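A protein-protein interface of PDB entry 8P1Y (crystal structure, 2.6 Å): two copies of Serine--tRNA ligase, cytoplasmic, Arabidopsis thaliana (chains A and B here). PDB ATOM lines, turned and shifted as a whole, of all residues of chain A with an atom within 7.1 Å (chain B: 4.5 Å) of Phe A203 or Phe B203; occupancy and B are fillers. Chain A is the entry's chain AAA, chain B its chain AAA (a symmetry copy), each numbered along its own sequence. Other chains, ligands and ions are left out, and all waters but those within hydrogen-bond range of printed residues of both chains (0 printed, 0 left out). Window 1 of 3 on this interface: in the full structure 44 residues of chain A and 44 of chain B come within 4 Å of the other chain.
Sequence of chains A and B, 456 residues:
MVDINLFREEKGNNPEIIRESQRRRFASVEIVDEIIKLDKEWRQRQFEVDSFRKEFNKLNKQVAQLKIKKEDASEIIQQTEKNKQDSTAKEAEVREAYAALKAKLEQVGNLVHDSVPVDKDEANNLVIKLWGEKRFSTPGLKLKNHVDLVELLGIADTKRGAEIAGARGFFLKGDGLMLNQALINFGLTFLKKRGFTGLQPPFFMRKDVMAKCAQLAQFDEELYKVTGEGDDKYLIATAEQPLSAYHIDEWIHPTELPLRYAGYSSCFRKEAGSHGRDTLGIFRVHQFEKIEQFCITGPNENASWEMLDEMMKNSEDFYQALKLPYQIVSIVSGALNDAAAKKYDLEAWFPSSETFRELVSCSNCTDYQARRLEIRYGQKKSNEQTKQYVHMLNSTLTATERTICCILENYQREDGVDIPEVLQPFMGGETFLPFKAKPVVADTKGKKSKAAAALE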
ATOM      1  N   ALA A 165      16.005  16.425   7.807  1.00  0.00           N
ATOM      2  CA  ALA A 165      15.874  16.056   9.240  1.00  0.00           C
ATOM      3  C   ALA A 165      16.918  15.006   9.624  1.00  0.00           C
ATOM      4  O   ALA A 165      16.886  14.548  10.789  1.00  0.00           O
ATOM      5  CB  ALA A 165      14.487  15.539   9.521  1.00  0.00           C
ATOM      6  N   PHE A 170      11.294  11.683   6.747  1.00  0.00           N
ATOM      7  CA  PHE A 170      10.355  11.591   5.598  1.00  0.00           C
ATOM      8  C   PHE A 170       9.427  12.819   5.577  1.00  0.00           C
ATOM      9  O   PHE A 170       9.058  13.352   6.663  1.00  0.00           O
ATOM     10  CB  PHE A 170       9.591  10.263   5.680  1.00  0.00           C
ATOM     11  CG  PHE A 170       8.770  10.059   6.934  1.00  0.00           C
ATOM     12  CD1 PHE A 170       9.318   9.490   8.077  1.00  0.00           C
ATOM     13  CD2 PHE A 170       7.435  10.422   6.977  1.00  0.00           C
ATOM     14  CE1 PHE A 170       8.553   9.298   9.224  1.00  0.00           C
ATOM     15  CE2 PHE A 170       6.677  10.235   8.125  1.00  0.00           C
ATOM     16  CZ  PHE A 170       7.232   9.663   9.245  1.00  0.00           C
ATOM     17  N   GLN A 200      -5.224  15.395  23.378  1.00  0.00           N
ATOM     18  CA  GLN A 200      -3.961  15.663  22.656  1.00  0.00           C
ATOM     19  C   GLN A 200      -3.035  16.295  23.682  1.00  0.00           C
ATOM     20  O   GLN A 200      -3.281  17.417  24.132  1.00  0.00           O
ATOM     21  CB  GLN A 200      -4.174  16.565  21.434  1.00  0.00           C
ATOM     22  CG  GLN A 200      -2.901  16.846  20.635  1.00  0.00           C
ATOM     23  CD  GLN A 200      -3.158  17.557  19.323  1.00  0.00           C
ATOM     24  OE1 GLN A 200      -4.254  17.521  18.760  1.00  0.00           O
ATOM     25  NE2 GLN A 200      -2.136  18.224  18.810  1.00  0.00           N
ATOM     26  N   PRO A 201      -1.959  15.589  24.096  1.00  0.00           N
ATOM     27  CA  PRO A 201      -1.014  16.153  25.047  1.00  0.00           C
ATOM     28  C   PRO A 201      -0.018  17.053  24.328  1.00  0.00           C
ATOM     29  O   PRO A 201       0.071  17.061  23.089  1.00  0.00           O
ATOM     30  CB  PRO A 201      -0.315  14.909  25.575  1.00  0.00           C
ATOM     31  CG  PRO A 201      -0.208  14.053  24.347  1.00  0.00           C
ATOM     32  CD  PRO A 201      -1.517  14.271  23.617  1.00  0.00           C
ATOM     33  N   PRO A 202       0.757  17.828  25.114  1.00  0.00           N
ATOM     34  CA  PRO A 202       1.963  18.478  24.605  1.00  0.00           C
ATOM     35  C   PRO A 202       3.047  17.434  24.282  1.00  0.00           C
ATOM     36  O   PRO A 202       3.142  16.435  25.010  1.00  0.00           O
ATOM     37  CB  PRO A 202       2.396  19.396  25.756  1.00  0.00           C
ATOM     38  CG  PRO A 202       1.237  19.404  26.749  1.00  0.00           C
ATOM     39  CD  PRO A 202       0.503  18.102  26.536  1.00  0.00           C
ATOM     40  N   PHE A 203       3.847  17.675  23.233  1.00  0.00           N
ATOM     41  CA  PHE A 203       4.977  16.796  22.817  1.00  0.00           C
ATOM     42  C   PHE A 203       6.227  17.077  23.665  1.00  0.00           C
ATOM     43  O   PHE A 203       7.261  16.453  23.393  1.00  0.00           O
ATOM     44  CB  PHE A 203       5.339  16.991  21.343  1.00  0.00           C
ATOM     45  CG  PHE A 203       4.211  16.932  20.344  1.00  0.00           C
ATOM     46  CD1 PHE A 203       2.967  16.401  20.672  1.00  0.00           C
ATOM     47  CD2 PHE A 203       4.428  17.370  19.044  1.00  0.00           C
ATOM     48  CE1 PHE A 203       1.950  16.360  19.731  1.00  0.00           C
ATOM     49  CE2 PHE A 203       3.421  17.308  18.097  1.00  0.00           C
ATOM     50  CZ  PHE A 203       2.183  16.813  18.447  1.00  0.00           C
ATOM     51  N   PHE A 204       6.136  18.033  24.605  1.00  0.00           N
ATOM     52  CA  PHE A 204       7.116  18.344  25.681  1.00  0.00           C
ATOM     53  C   PHE A 204       6.660  17.744  27.019  1.00  0.00           C
ATOM     54  O   PHE A 204       5.457  17.747  27.339  1.00  0.00           O
ATOM     55  CB  PHE A 204       7.261  19.857  25.884  1.00  0.00           C
ATOM     56  CG  PHE A 204       7.829  20.640  24.727  1.00  0.00           C
ATOM     57  CD1 PHE A 204       8.430  20.014  23.640  1.00  0.00           C
ATOM     58  CD2 PHE A 204       7.795  22.024  24.745  1.00  0.00           C
ATOM     59  CE1 PHE A 204       8.961  20.755  22.591  1.00  0.00           C
ATOM     60  CE2 PHE A 204       8.320  22.764  23.695  1.00  0.00           C
ATOM     61  CZ  PHE A 204       8.903  22.129  22.620  1.00  0.00           C
ATOM     62  N   MET A 205       7.620  17.266  27.810  1.00  0.00           N
ATOM     63  CA  MET A 205       7.418  16.937  29.243  1.00  0.00           C
ATOM     64  C   MET A 205       8.688  17.278  30.018  1.00  0.00           C
ATOM     65  O   MET A 205       9.784  16.912  29.549  1.00  0.00           O
ATOM     66  CB  MET A 205       7.087  15.460  29.445  1.00  0.00           C
ATOM     67  CG  MET A 205       6.454  15.180  30.791  1.00  0.00           C
ATOM     68  SD  MET A 205       5.949  13.461  30.971  1.00  0.00           S
ATOM     69  CE  MET A 205       5.075  13.218  29.427  1.00  0.00           C
ATOM     70  N   VAL A 226      15.101  18.373  24.835  1.00  0.00           N
ATOM     71  CA  VAL A 226      14.717  19.715  24.297  1.00  0.00           C
ATOM     72  C   VAL A 226      15.214  20.818  25.243  1.00  0.00           C
ATOM     73  O   VAL A 226      14.673  20.929  26.353  1.00  0.00           O
ATOM     74  CB  VAL A 226      13.198  19.814  24.073  1.00  0.00           C
ATOM     75  CG1 VAL A 226      12.835  21.079  23.312  1.00  0.00           C
ATOM     76  CG2 VAL A 226      12.656  18.592  23.356  1.00  0.00           C
ATOM     77  N   LYS A 233      13.668  19.505  28.862  1.00  0.00           N
ATOM     78  CA  LYS A 233      12.452  18.713  28.546  1.00  0.00           C
ATOM     79  C   LYS A 233      12.839  17.549  27.629  1.00  0.00           C
ATOM     80  O   LYS A 233      13.883  17.633  26.948  1.00  0.00           O
ATOM     81  CB  LYS A 233      11.402  19.575  27.833  1.00  0.00           C
ATOM     82  CG  LYS A 233      11.106  20.940  28.450  1.00  0.00           C
ATOM     83  CD  LYS A 233      10.874  22.040  27.421  1.00  0.00           C
ATOM     84  CE  LYS A 233      10.908  23.437  28.004  1.00  0.00           C
ATOM     85  NZ  LYS A 233      10.024  23.554  29.188  1.00  0.00           N
ATOM     86  N   TYR A 234      12.000  16.516  27.607  1.00  0.00           N
ATOM     87  CA  TYR A 234      12.043  15.402  26.630  1.00  0.00           C
ATOM     88  C   TYR A 234      10.935  15.608  25.586  1.00  0.00           C
ATOM     89  O   TYR A 234       9.887  16.182  25.943  1.00  0.00           O
ATOM     90  CB  TYR A 234      11.845  14.070  27.354  1.00  0.00           C
ATOM     91  CG  TYR A 234      12.938  13.674  28.318  1.00  0.00           C
ATOM     92  CD1 TYR A 234      14.253  13.535  27.895  1.00  0.00           C
ATOM     93  CD2 TYR A 234      12.649  13.378  29.643  1.00  0.00           C
ATOM     94  CE1 TYR A 234      15.254  13.139  28.769  1.00  0.00           C
ATOM     95  CE2 TYR A 234      13.635  12.975  30.528  1.00  0.00           C
ATOM     96  CZ  TYR A 234      14.944  12.857  30.088  1.00  0.00           C
ATOM     97  OH  TYR A 234      15.930  12.470  30.947  1.00  0.00           O
ATOM     98  N   LEU A 235      11.167  15.169  24.339  1.00  0.00           N
ATOM     99  CA  LEU A 235      10.093  14.820  23.368  1.00  0.00           C
ATOM    100  C   LEU A 235       9.488  13.481  23.810  1.00  0.00           C
ATOM    101  O   LEU A 235      10.272  12.543  24.120  1.00  0.00           O
ATOM    102  CB  LEU A 235      10.656  14.744  21.942  1.00  0.00           C
ATOM    103  CG  LEU A 235      11.107  16.067  21.314  1.00  0.00           C
ATOM    104  CD1 LEU A 235      11.643  15.876  19.898  1.00  0.00           C
ATOM    105  CD2 LEU A 235       9.979  17.081  21.291  1.00  0.00           C
ATOM    106  N   ILE A 236       8.155  13.399  23.896  1.00  0.00           N
ATOM    107  CA  ILE A 236       7.437  12.151  24.300  1.00  0.00           C
ATOM    108  C   ILE A 236       7.751  11.062  23.267  1.00  0.00           C
ATOM    109  O   ILE A 236       7.836  11.383  22.058  1.00  0.00           O
ATOM    110  CB  ILE A 236       5.920  12.380  24.487  1.00  0.00           C
ATOM    111  CG1 ILE A 236       5.224  12.869  23.209  1.00  0.00           C
ATOM    112  CG2 ILE A 236       5.675  13.317  25.658  1.00  0.00           C
ATOM    113  CD1 ILE A 236       3.712  12.984  23.315  1.00  0.00           C
ATOM    114  N   ALA A 237       7.976   9.835  23.741  1.00  0.00           N
ATOM    115  CA  ALA A 237       8.088   8.606  22.917  1.00  0.00           C
ATOM    116  C   ALA A 237       6.691   8.063  22.583  1.00  0.00           C
ATOM    117  O   ALA A 237       6.530   7.453  21.500  1.00  0.00           O
ATOM    118  CB  ALA A 237       8.909   7.563  23.639  1.00  0.00           C
ATOM    119  N   PRO A 242       2.397  11.321  28.740  1.00  0.00           N
ATOM    120  CA  PRO A 242       1.741  12.536  29.210  1.00  0.00           C
ATOM    121  C   PRO A 242       0.411  12.197  29.893  1.00  0.00           C
ATOM    122  O   PRO A 242       0.146  12.726  30.959  1.00  0.00           O
ATOM    123  CB  PRO A 242       1.536  13.394  27.952  1.00  0.00           C
ATOM    124  CG  PRO A 242       1.824  12.475  26.774  1.00  0.00           C
ATOM    125  CD  PRO A 242       2.713  11.376  27.307  1.00  0.00           C
ATOM    126  N   TYR A 264      -4.088  11.254  21.367  1.00  0.00           N
ATOM    127  CA  TYR A 264      -3.456  11.511  20.053  1.00  0.00           C
ATOM    128  C   TYR A 264      -2.249  12.437  20.194  1.00  0.00           C
ATOM    129  O   TYR A 264      -2.416  13.478  20.809  1.00  0.00           O
ATOM    130  CB  TYR A 264      -4.441  12.152  19.084  1.00  0.00           C
ATOM    131  CG  TYR A 264      -3.782  12.685  17.837  1.00  0.00           C
ATOM    132  CD1 TYR A 264      -3.070  11.850  17.000  1.00  0.00           C
ATOM    133  CD2 TYR A 264      -3.831  14.032  17.520  1.00  0.00           C
ATOM    134  CE1 TYR A 264      -2.443  12.332  15.865  1.00  0.00           C
ATOM    135  CE2 TYR A 264      -3.231  14.526  16.376  1.00  0.00           C
ATOM    136  CZ  TYR A 264      -2.535  13.673  15.546  1.00  0.00           C
ATOM    137  OH  TYR A 264      -1.940  14.151  14.413  1.00  0.00           O
ATOM    138  N   SER A 265      -1.117  12.085  19.564  1.00  0.00           N
ATOM    139  CA  SER A 265       0.109  12.920  19.446  1.00  0.00           C
ATOM    140  C   SER A 265       1.026  12.435  18.311  1.00  0.00           C
ATOM    141  O   SER A 265       0.895  11.268  17.873  1.00  0.00           O
ATOM    142  CB  SER A 265       0.848  12.887  20.729  1.00  0.00           C
ATOM    143  OG  SER A 265       0.901  11.549  21.206  1.00  0.00           O
ATOM    144  N   SER A 266       1.927  13.319  17.870  1.00  0.00           N
ATOM    145  CA  SER A 266       3.229  12.984  17.239  1.00  0.00           C
ATOM    146  C   SER A 266       4.142  12.283  18.271  1.00  0.00           C
ATOM    147  O   SER A 266       4.050  12.589  19.485  1.00  0.00           O
ATOM    148  CB  SER A 266       3.875  14.221  16.660  1.00  0.00           C
ATOM    149  OG  SER A 266       3.560  14.352  15.277  1.00  0.00           O
ATOM    150  N   CYS A 267       5.002  11.363  17.818  1.00  0.00           N
ATOM    151  CA  CYS A 267       5.865  10.519  18.685  1.00  0.00           C
ATOM    152  C   CYS A 267       7.295  10.489  18.143  1.00  0.00           C
ATOM    153  O   CYS A 267       7.460  10.304  16.919  1.00  0.00           O
ATOM    154  CB  CYS A 267       5.322   9.100  18.785  1.00  0.00           C
ATOM    155  SG  CYS A 267       3.857   8.977  19.840  1.00  0.00           S
ATOM    156  N   PHE A 268       8.271  10.627  19.050  1.00  0.00           N
ATOM    157  CA  PHE A 268       9.730  10.723  18.770  1.00  0.00           C
ATOM    158  C   PHE A 268      10.454   9.602  19.529  1.00  0.00           C
ATOM    159  O   PHE A 268      10.318   9.500  20.763  1.00  0.00           O
ATOM    160  CB  PHE A 268      10.226  12.134  19.103  1.00  0.00           C
ATOM    161  CG  PHE A 268       9.321  13.219  18.575  1.00  0.00           C
ATOM    162  CD1 PHE A 268       8.214  13.645  19.307  1.00  0.00           C
ATOM    163  CD2 PHE A 268       9.539  13.781  17.325  1.00  0.00           C
ATOM    164  CE1 PHE A 268       7.351  14.612  18.806  1.00  0.00           C
ATOM    165  CE2 PHE A 268       8.675  14.749  16.827  1.00  0.00           C
ATOM    166  CZ  PHE A 268       7.588  15.166  17.570  1.00  0.00           C
ATOM    167  N   GLN A 287      10.212   9.994  13.968  1.00  0.00           N
ATOM    168  CA  GLN A 287       8.943  10.729  14.217  1.00  0.00           C
ATOM    169  C   GLN A 287       7.774   9.975  13.576  1.00  0.00           C
ATOM    170  O   GLN A 287       7.938   9.485  12.440  1.00  0.00           O
ATOM    171  CB  GLN A 287       9.024  12.139  13.640  1.00  0.00           C
ATOM    172  CG  GLN A 287       7.796  12.980  13.948  1.00  0.00           C
ATOM    173  CD  GLN A 287       7.688  14.197  13.064  1.00  0.00           C
ATOM    174  OE1 GLN A 287       6.586  14.621  12.723  1.00  0.00           O
ATOM    175  NE2 GLN A 287       8.830  14.748  12.674  1.00  0.00           N
ATOM    176  N   PHE A 288       6.631   9.912  14.264  1.00  0.00           N
ATOM    177  CA  PHE A 288       5.382   9.264  13.774  1.00  0.00           C
ATOM    178  C   PHE A 288       4.198   9.679  14.675  1.00  0.00           C
ATOM    179  O   PHE A 288       4.442  10.225  15.774  1.00  0.00           O
ATOM    180  CB  PHE A 288       5.598   7.745  13.685  1.00  0.00           C
ATOM    181  CG  PHE A 288       6.008   7.096  14.984  1.00  0.00           C
ATOM    182  CD1 PHE A 288       5.052   6.597  15.856  1.00  0.00           C
ATOM    183  CD2 PHE A 288       7.343   7.021  15.352  1.00  0.00           C
ATOM    184  CE1 PHE A 288       5.421   6.045  17.073  1.00  0.00           C
ATOM    185  CE2 PHE A 288       7.713   6.469  16.566  1.00  0.00           C
ATOM    186  CZ  PHE A 288       6.754   5.977  17.422  1.00  0.00           C
ATOM    187  N   GLU A 289       2.951   9.452  14.226  1.00  0.00           N
ATOM    188  CA  GLU A 289       1.724   9.759  15.012  1.00  0.00           C
ATOM    189  C   GLU A 289       1.073   8.457  15.481  1.00  0.00           C
ATOM    190  O   GLU A 289       1.239   7.414  14.828  1.00  0.00           O
ATOM    191  CB  GLU A 289       0.681  10.559  14.231  1.00  0.00           C
ATOM    192  CG  GLU A 289       1.211  11.828  13.617  1.00  0.00           C
ATOM    193  CD  GLU A 289       2.322  11.561  12.620  1.00  0.00           C
ATOM    194  OE1 GLU A 289       2.027  11.033  11.544  1.00  0.00           O
ATOM    195  OE2 GLU A 289       3.491  11.836  12.954  1.00  0.00           O
ATOM    196  N   PRO B 201       6.212  18.055   6.506  1.00  0.00           N
ATOM    197  CA  PRO B 201       7.643  17.915   6.718  1.00  0.00           C
ATOM    198  C   PRO B 201       7.912  17.242   8.057  1.00  0.00           C
ATOM    199  O   PRO B 201       7.012  17.089   8.898  1.00  0.00           O
ATOM    200  CB  PRO B 201       8.101  19.366   6.756  1.00  0.00           C
ATOM    201  CG  PRO B 201       6.976  20.040   7.486  1.00  0.00           C
ATOM    202  CD  PRO B 201       5.725  19.365   6.963  1.00  0.00           C
ATOM    203  N   PRO B 202       9.180  16.831   8.270  1.00  0.00           N
ATOM    204  CA  PRO B 202       9.662  16.482   9.605  1.00  0.00           C
ATOM    205  C   PRO B 202       9.741  17.734  10.497  1.00  0.00           C
ATOM    206  O   PRO B 202      10.075  18.809   9.979  1.00  0.00           O
ATOM    207  CB  PRO B 202      11.053  15.890   9.348  1.00  0.00           C
ATOM    208  CG  PRO B 202      11.156  15.693   7.837  1.00  0.00           C
ATOM    209  CD  PRO B 202      10.206  16.695   7.226  1.00  0.00           C
ATOM    210  N   PHE B 203       9.459  17.586  11.800  1.00  0.00           N
ATOM    211  CA  PHE B 203       9.539  18.681  12.808  1.00  0.00           C
ATOM    212  C   PHE B 203      10.988  18.881  13.281  1.00  0.00           C
ATOM    213  O   PHE B 203      11.196  19.727  14.161  1.00  0.00           O
ATOM    214  CB  PHE B 203       8.666  18.394  14.033  1.00  0.00           C
ATOM    215  CG  PHE B 203       7.235  17.996  13.778  1.00  0.00           C
ATOM    216  CD1 PHE B 203       6.625  18.196  12.543  1.00  0.00           C
ATOM    217  CD2 PHE B 203       6.481  17.462  14.816  1.00  0.00           C
ATOM    218  CE1 PHE B 203       5.306  17.820  12.341  1.00  0.00           C
ATOM    219  CE2 PHE B 203       5.158  17.108  14.623  1.00  0.00           C
ATOM    220  CZ  PHE B 203       4.578  17.279  13.383  1.00  0.00           C
ATOM    221  N   PHE B 204      11.927  18.077  12.757  1.00  0.00           N
ATOM    222  CA  PHE B 204      13.405  18.205  12.884  1.00  0.00           C
ATOM    223  C   PHE B 204      14.005  18.830  11.616  1.00  0.00           C
ATOM    224  O   PHE B 204      13.563  18.534  10.491  1.00  0.00           O
ATOM    225  CB  PHE B 204      14.069  16.836  13.076  1.00  0.00           C
ATOM    226  CG  PHE B 204      13.724  16.093  14.343  1.00  0.00           C
ATOM    227  CD1 PHE B 204      13.055  16.707  15.397  1.00  0.00           C
ATOM    228  CD2 PHE B 204      14.107  14.771  14.495  1.00  0.00           C
ATOM    229  CE1 PHE B 204      12.760  16.008  16.561  1.00  0.00           C
ATOM    230  CE2 PHE B 204      13.807  14.071  15.656  1.00  0.00           C
ATOM    231  CZ  PHE B 204      13.135  14.690  16.688  1.00  0.00           C
ATOM    232  N   MET B 205      15.030  19.662  11.797  1.00  0.00           N
ATOM    233  CA  MET B 205      15.926  20.115  10.703  1.00  0.00           C
ATOM    234  C   MET B 205      17.346  20.254  11.245  1.00  0.00           C
ATOM    235  O   MET B 205      17.509  20.846  12.330  1.00  0.00           O
ATOM    236  CB  MET B 205      15.476  21.453  10.119  1.00  0.00           C
ATOM    237  CG  MET B 205      16.071  21.726   8.755  1.00  0.00           C
ATOM    238  SD  MET B 205      15.438  23.242   8.017  1.00  0.00           S
ATOM    239  CE  MET B 205      13.680  23.015   8.273  1.00  0.00           C
ATOM    240  N   TYR B 234      17.173  21.577  15.193  1.00  0.00           N
ATOM    241  CA  TYR B 234      16.132  22.513  15.681  1.00  0.00           C
ATOM    242  C   TYR B 234      14.752  21.863  15.507  1.00  0.00           C
ATOM    243  O   TYR B 234      14.587  21.072  14.556  1.00  0.00           O
ATOM    244  CB  TYR B 234      16.202  23.822  14.895  1.00  0.00           C
ATOM    245  CG  TYR B 234      17.459  24.638  15.081  1.00  0.00           C
ATOM    246  CD1 TYR B 234      17.849  25.081  16.338  1.00  0.00           C
ATOM    247  CD2 TYR B 234      18.231  25.019  13.992  1.00  0.00           C
ATOM    248  CE1 TYR B 234      18.983  25.859  16.510  1.00  0.00           C
ATOM    249  CE2 TYR B 234      19.364  25.801  14.145  1.00  0.00           C
ATOM    250  CZ  TYR B 234      19.742  26.220  15.410  1.00  0.00           C
ATOM    251  OH  TYR B 234      20.860  26.983  15.581  1.00  0.00           O
ATOM    252  N   LEU B 235      13.801  22.174  16.402  1.00  0.00           N
ATOM    253  CA  LEU B 235      12.340  22.070  16.133  1.00  0.00           C
ATOM    254  C   LEU B 235      11.958  23.233  15.207  1.00  0.00           C
ATOM    255  O   LEU B 235      12.382  24.387  15.489  1.00  0.00           O
ATOM    256  CB  LEU B 235      11.543  22.104  17.445  1.00  0.00           C
ATOM    257  CG  LEU B 235      11.690  20.887  18.365  1.00  0.00           C
ATOM    258  CD1 LEU B 235      10.853  21.025  19.633  1.00  0.00           C
ATOM    259  CD2 LEU B 235      11.311  19.604  17.650  1.00  0.00           C
ATOM    260  N   ILE B 236      11.237  22.948  14.116  1.00  0.00           N
ATOM    261  CA  ILE B 236      10.786  23.987  13.140  1.00  0.00           C
ATOM    262  C   ILE B 236       9.865  24.968  13.876  1.00  0.00           C
ATOM    263  O   ILE B 236       9.073  24.520  14.738  1.00  0.00           O
ATOM    264  CB  ILE B 236      10.125  23.370  11.887  1.00  0.00           C
ATOM    265  CG1 ILE B 236       8.880  22.534  12.214  1.00  0.00           C
ATOM    266  CG2 ILE B 236      11.150  22.572  11.097  1.00  0.00           C
ATOM    267  CD1 ILE B 236       8.127  22.015  11.000  1.00  0.00           C
ATOM    268  N   SER B 265       2.220  20.997   9.496  1.00  0.00           N
ATOM    269  CA  SER B 265       3.066  20.532  10.628  1.00  0.00           C
ATOM    270  C   SER B 265       2.581  21.094  11.975  1.00  0.00           C
ATOM    271  O   SER B 265       1.841  22.105  11.987  1.00  0.00           O
ATOM    272  CB  SER B 265       4.468  20.946  10.394  1.00  0.00           C
ATOM    273  OG  SER B 265       4.490  22.298   9.953  1.00  0.00           O
ATOM    274  N   SER B 266       3.006  20.446  13.065  1.00  0.00           N
ATOM    275  CA  SER B 266       3.172  21.043  14.414  1.00  0.00           C
ATOM    276  C   SER B 266       4.293  22.108  14.378  1.00  0.00           C
ATOM    277  O   SER B 266       5.261  21.958  13.593  1.00  0.00           O
ATOM    278  CB  SER B 266       3.444  19.970  15.443  1.00  0.00           C
ATOM    279  OG  SER B 266       2.236  19.568  16.080  1.00  0.00           O
ATOM    280  N   PHE B 268       6.794  24.947  16.844  1.00  0.00           N
ATOM    281  CA  PHE B 268       7.441  25.227  18.155  1.00  0.00           C
ATOM    282  C   PHE B 268       8.126  26.600  18.085  1.00  0.00           C
ATOM    283  O   PHE B 268       8.969  26.828  17.198  1.00  0.00           O
ATOM    284  CB  PHE B 268       8.378  24.073  18.523  1.00  0.00           C
ATOM    285  CG  PHE B 268       7.758  22.715  18.305  1.00  0.00           C
ATOM    286  CD1 PHE B 268       7.806  22.100  17.055  1.00  0.00           C
ATOM    287  CD2 PHE B 268       7.078  22.070  19.329  1.00  0.00           C
ATOM    288  CE1 PHE B 268       7.198  20.871  16.835  1.00  0.00           C
ATOM    289  CE2 PHE B 268       6.472  20.840  19.107  1.00  0.00           C
ATOM    290  CZ  PHE B 268       6.538  20.241  17.864  1.00  0.00           C
ATOM    291  N   GLN B 287       3.815  25.396  21.419  1.00  0.00           N
ATOM    292  CA  GLN B 287       3.487  24.374  20.388  1.00  0.00           C
ATOM    293  C   GLN B 287       2.111  24.675  19.783  1.00  0.00           C
ATOM    294  O   GLN B 287       1.193  25.030  20.549  1.00  0.00           O
ATOM    295  CB  GLN B 287       3.484  22.979  21.003  1.00  0.00           C
ATOM    296  CG  GLN B 287       3.254  21.878  19.981  1.00  0.00           C
ATOM    297  CD  GLN B 287       2.854  20.570  20.616  1.00  0.00           C
ATOM    298  OE1 GLN B 287       2.078  19.810  20.039  1.00  0.00           O
ATOM    299  NE2 GLN B 287       3.362  20.313  21.814  1.00  0.00           N
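The backbone NH (N) of Phe A203 lies close to the side-chain amide nitrogen (NE2) of Gln B287.
N of Phe B203 lies close to NE2 of Gln A287, at 3.0 Å.
O of Phe A203 lies within hydrogen-bond range of N of Ile A236 (3.2 Å).
N of Phe A268 is in hydrogen-bond range of O of Ile A236 (3.1 Å).
The side-chain hydroxyl (OG) of Ser A266 sits at hydrogen-bond distance from the side-chain carboxylate (OE2) of Glu A289 (3.4 Å).
The backbone carbonyl oxygen (O) of Phe B203 lies within hydrogen-bond range of the backbone NH (N) of Ile B236, 3.2 Å away.
The backbone carbonyl oxygen (O) of Ile B236 lies within hydrogen-bond range of the backbone NH (N) of Phe B268, at 3.1 Å.
Ala A165 touches Pro B202.
Ala A165 touches Phe B204.
Phe A170 touches Pro B202 (O to CG, 3.4 Å).
Pro A202 touches Gln B287.
Phe A203 touches Phe B203.
CE2 of Phe A203 touches OG of Ser B266 (3.3 Å).
CD1 of Leu B235 touches CE1 of Phe A204, 3.5 Å away.
CZ of Phe A204 touches CD2 of Phe B268, at 3.8 Å.
Phe B203 touches Ser A266.
Phe A268 touches Phe B204.
Pro A201 touches none of the printed residues of chain B.
Cys A267 touches none of the printed residues of chain B.
Of chain A, only Phe A203 (3.9 Å), Ser A266 (3.3 Å), Phe A268 (3.8 Å) and Gln A287 (3.0 Å) come within 4 Å of Phe B203.
Of the printed residues of chain A, Leu B235 touches Phe A204 (3.5 Å).
Of the printed residues of chain A, Ser B266 touches Phe A203 (3.3 Å).
The nearest printed residue of chain B that does not touch Phe A203 is Leu B235 (6.9 Å).
The nearest printed residue of chain A that does not touch Pro B202 is Phe A268 (7.1 Å).
Printed residues of chain A that touch a printed residue of chain B: Ala A165, Phe A170, Pro A202, Phe A203, Phe A204, Leu A235, Ser A266, Phe A268 and Gln A287.
Hydrophobic or aromatic side chains of chain A that line the printed part of chain B: Ala A165, Phe A203, Phe A204, Leu A235 and Phe A268.
Printed residues of chain B that touch a printed residue of chain A: Pro B202, Phe B203, Phe B204, Leu B235, Ser B266, Phe B268 and Gln B287.
Among the printed residues, no Asp or Glu carboxylate lies within 4 Å of a Lys or Arg side-chain nitrogen of the other chain.
Pro A202 touches Gln B287, and with the chains exchanged Gln A287 touches Pro B202.
Phe A203 touches Ser B266, and with the chains exchanged Ser A266 touches Phe B203.
Phe A204 touches Leu B235, and with the chains exchanged Leu A235 touches Phe B204.
Phe A204 touches Phe B268, and with the chains exchanged Phe A268 touches Phe B204.
Of the 16 pairs that touch across the chains among the printed residues, 13 have their exchanged pair printed and touching as well.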
